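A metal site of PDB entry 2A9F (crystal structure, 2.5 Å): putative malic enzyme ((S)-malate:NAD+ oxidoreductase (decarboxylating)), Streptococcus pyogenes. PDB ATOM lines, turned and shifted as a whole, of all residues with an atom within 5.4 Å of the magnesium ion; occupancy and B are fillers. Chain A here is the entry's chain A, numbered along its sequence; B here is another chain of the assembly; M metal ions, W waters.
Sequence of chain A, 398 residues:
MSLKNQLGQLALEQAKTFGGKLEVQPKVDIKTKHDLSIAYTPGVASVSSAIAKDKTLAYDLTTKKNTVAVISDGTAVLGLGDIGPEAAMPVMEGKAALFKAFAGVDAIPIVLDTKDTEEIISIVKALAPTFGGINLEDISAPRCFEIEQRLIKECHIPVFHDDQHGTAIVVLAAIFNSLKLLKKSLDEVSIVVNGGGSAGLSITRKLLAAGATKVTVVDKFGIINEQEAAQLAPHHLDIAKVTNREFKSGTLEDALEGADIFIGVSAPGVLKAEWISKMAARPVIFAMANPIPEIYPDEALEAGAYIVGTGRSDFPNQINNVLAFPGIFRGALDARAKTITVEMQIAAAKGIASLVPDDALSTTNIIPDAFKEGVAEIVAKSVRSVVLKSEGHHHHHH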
ATOM      1  N   LEU A  78     -11.625 -26.526 -22.952  1.00  0.00           N
ATOM      2  CA  LEU A  78     -11.788 -27.883 -23.471  1.00  0.00           C
ATOM      3  C   LEU A  78     -10.718 -28.368 -24.478  1.00  0.00           C
ATOM      4  O   LEU A  78      -9.527 -28.406 -24.178  1.00  0.00           O
ATOM      5  CB  LEU A  78     -13.194 -28.034 -24.089  1.00  0.00           C
ATOM      6  CG  LEU A  78     -14.390 -28.446 -23.222  1.00  0.00           C
ATOM      7  CD1 LEU A  78     -14.249 -27.907 -21.828  1.00  0.00           C
ATOM      8  CD2 LEU A  78     -15.690 -27.930 -23.866  1.00  0.00           C
ATOM      9  N   LYS A  95     -19.800 -26.338 -15.902  1.00  0.00           N
ATOM     10  CA  LYS A  95     -19.001 -26.890 -14.839  1.00  0.00           C
ATOM     11  C   LYS A  95     -19.657 -26.576 -13.495  1.00  0.00           C
ATOM     12  O   LYS A  95     -19.677 -27.420 -12.595  1.00  0.00           O
ATOM     13  CB  LYS A  95     -17.595 -26.296 -14.886  1.00  0.00           C
ATOM     14  CG  LYS A  95     -16.576 -27.013 -14.008  1.00  0.00           C
ATOM     15  CD  LYS A  95     -16.124 -28.315 -14.646  1.00  0.00           C
ATOM     16  CE  LYS A  95     -14.849 -28.836 -14.002  1.00  0.00           C
ATOM     17  NZ  LYS A  95     -14.183 -29.815 -14.918  1.00  0.00           N
ATOM     18  N   GLU A 137     -10.012 -23.162 -13.946  1.00  0.00           N
ATOM     19  CA  GLU A 137     -10.379 -24.047 -15.042  1.00  0.00           C
ATOM     20  C   GLU A 137      -9.934 -23.611 -16.426  1.00  0.00           C
ATOM     21  O   GLU A 137      -9.960 -22.431 -16.769  1.00  0.00           O
ATOM     22  CB  GLU A 137     -11.898 -24.239 -15.060  1.00  0.00           C
ATOM     23  CG  GLU A 137     -12.413 -25.292 -16.042  1.00  0.00           C
ATOM     24  CD  GLU A 137     -12.255 -26.722 -15.521  1.00  0.00           C
ATOM     25  OE1 GLU A 137     -12.449 -26.931 -14.295  1.00  0.00           O
ATOM     26  OE2 GLU A 137     -11.973 -27.625 -16.331  1.00  0.00           O
ATOM     27  N   ASP A 138      -9.532 -24.589 -17.212  1.00  0.00           N
ATOM     28  CA  ASP A 138      -9.109 -24.375 -18.575  1.00  0.00           C
ATOM     29  C   ASP A 138      -8.146 -23.224 -18.850  1.00  0.00           C
ATOM     30  O   ASP A 138      -8.270 -22.543 -19.860  1.00  0.00           O
ATOM     31  CB  ASP A 138     -10.342 -24.226 -19.471  1.00  0.00           C
ATOM     32  CG  ASP A 138     -11.217 -25.468 -19.465  1.00  0.00           C
ATOM     33  OD1 ASP A 138     -10.810 -26.507 -18.883  1.00  0.00           O
ATOM     34  OD2 ASP A 138     -12.317 -25.411 -20.063  1.00  0.00           O
ATOM     35  N   ASP A 162      -8.445 -27.745 -11.514  1.00  0.00           N
ATOM     36  CA  ASP A 162      -9.056 -29.027 -11.832  1.00  0.00           C
ATOM     37  C   ASP A 162      -8.505 -29.786 -13.028  1.00  0.00           C
ATOM     38  O   ASP A 162      -8.333 -30.994 -12.946  1.00  0.00           O
ATOM     39  CB  ASP A 162     -10.558 -28.848 -11.957  1.00  0.00           C
ATOM     40  CG  ASP A 162     -11.267 -30.148 -12.107  1.00  0.00           C
ATOM     41  OD1 ASP A 162     -11.513 -30.555 -13.252  1.00  0.00           O
ATOM     42  OD2 ASP A 162     -11.563 -30.781 -11.059  1.00  0.00           O
ATOM     43  N   ASP A 163      -8.229 -29.096 -14.120  1.00  0.00           N
ATOM     44  CA  ASP A 163      -7.722 -29.741 -15.325  1.00  0.00           C
ATOM     45  C   ASP A 163      -6.376 -30.450 -15.138  1.00  0.00           C
ATOM     46  O   ASP A 163      -5.803 -30.962 -16.093  1.00  0.00           O
ATOM     47  CB  ASP A 163      -7.608 -28.715 -16.461  1.00  0.00           C
ATOM     48  CG  ASP A 163      -8.956 -28.260 -16.974  1.00  0.00           C
ATOM     49  OD1 ASP A 163      -9.677 -29.076 -17.600  1.00  0.00           O
ATOM     50  OD2 ASP A 163      -9.313 -27.080 -16.759  1.00  0.00           O
ATOM     51  N   TYR B  40     -22.979 -30.189 -20.908  1.00  0.00           N
ATOM     52  CA  TYR B  40     -21.543 -30.220 -20.764  1.00  0.00           C
ATOM     53  C   TYR B  40     -20.928 -30.887 -21.992  1.00  0.00           C
ATOM     54  O   TYR B  40     -21.497 -30.852 -23.081  1.00  0.00           O
ATOM     55  CB  TYR B  40     -21.129 -30.955 -19.490  1.00  0.00           C
ATOM     56  CG  TYR B  40     -19.775 -30.509 -18.971  1.00  0.00           C
ATOM     57  CD1 TYR B  40     -19.486 -29.144 -18.797  1.00  0.00           C
ATOM     58  CD2 TYR B  40     -18.778 -31.427 -18.684  1.00  0.00           C
ATOM     59  CE1 TYR B  40     -18.230 -28.718 -18.364  1.00  0.00           C
ATOM     60  CE2 TYR B  40     -17.522 -31.018 -18.237  1.00  0.00           C
ATOM     61  CZ  TYR B  40     -17.257 -29.664 -18.084  1.00  0.00           C
ATOM     62  OH  TYR B  40     -16.009 -29.241 -17.669  1.00  0.00           O
HETATM   63 MG    MG M   1     -11.444 -28.265 -18.111  1.00  0.00          MG
HETATM   64  O   HOH W   1     -13.104 -27.682 -19.035  1.00  0.00           O
HETATM   65  O   HOH W   2     -10.491 -29.293 -19.769  1.00  0.00           O
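The side-chain carboxylate (OE2) of Glu 137 binds the magnesium ion (2.0 Å).
Water W1 binds the magnesium ion.
OD1 of Asp 163 is bound to the magnesium ion (2.0 Å).
The side-chain carboxylate (OD1) of Asp 138 is bound to the magnesium ion, at 2.0 Å.
Water W2 binds the magnesium ion, at 2.2 Å.
Slightly farther from the magnesium ion lies OD2 of Asp 163 (2.8 Å).
Three residues have an atom within 4 Å of the magnesium ion: Glu 137, Asp 138 and Asp 163.
The nearest printed residue that does not touch the magnesium ion is Lys 95 (4.5 Å).
OD2 of Asp 138 lies within hydrogen-bond range of N of Leu 78 (3.2 Å).
The side-chain carboxylate of Glu 137 lies within salt-bridge range of the side-chain amino group of Lys 95 (3.4 Å).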
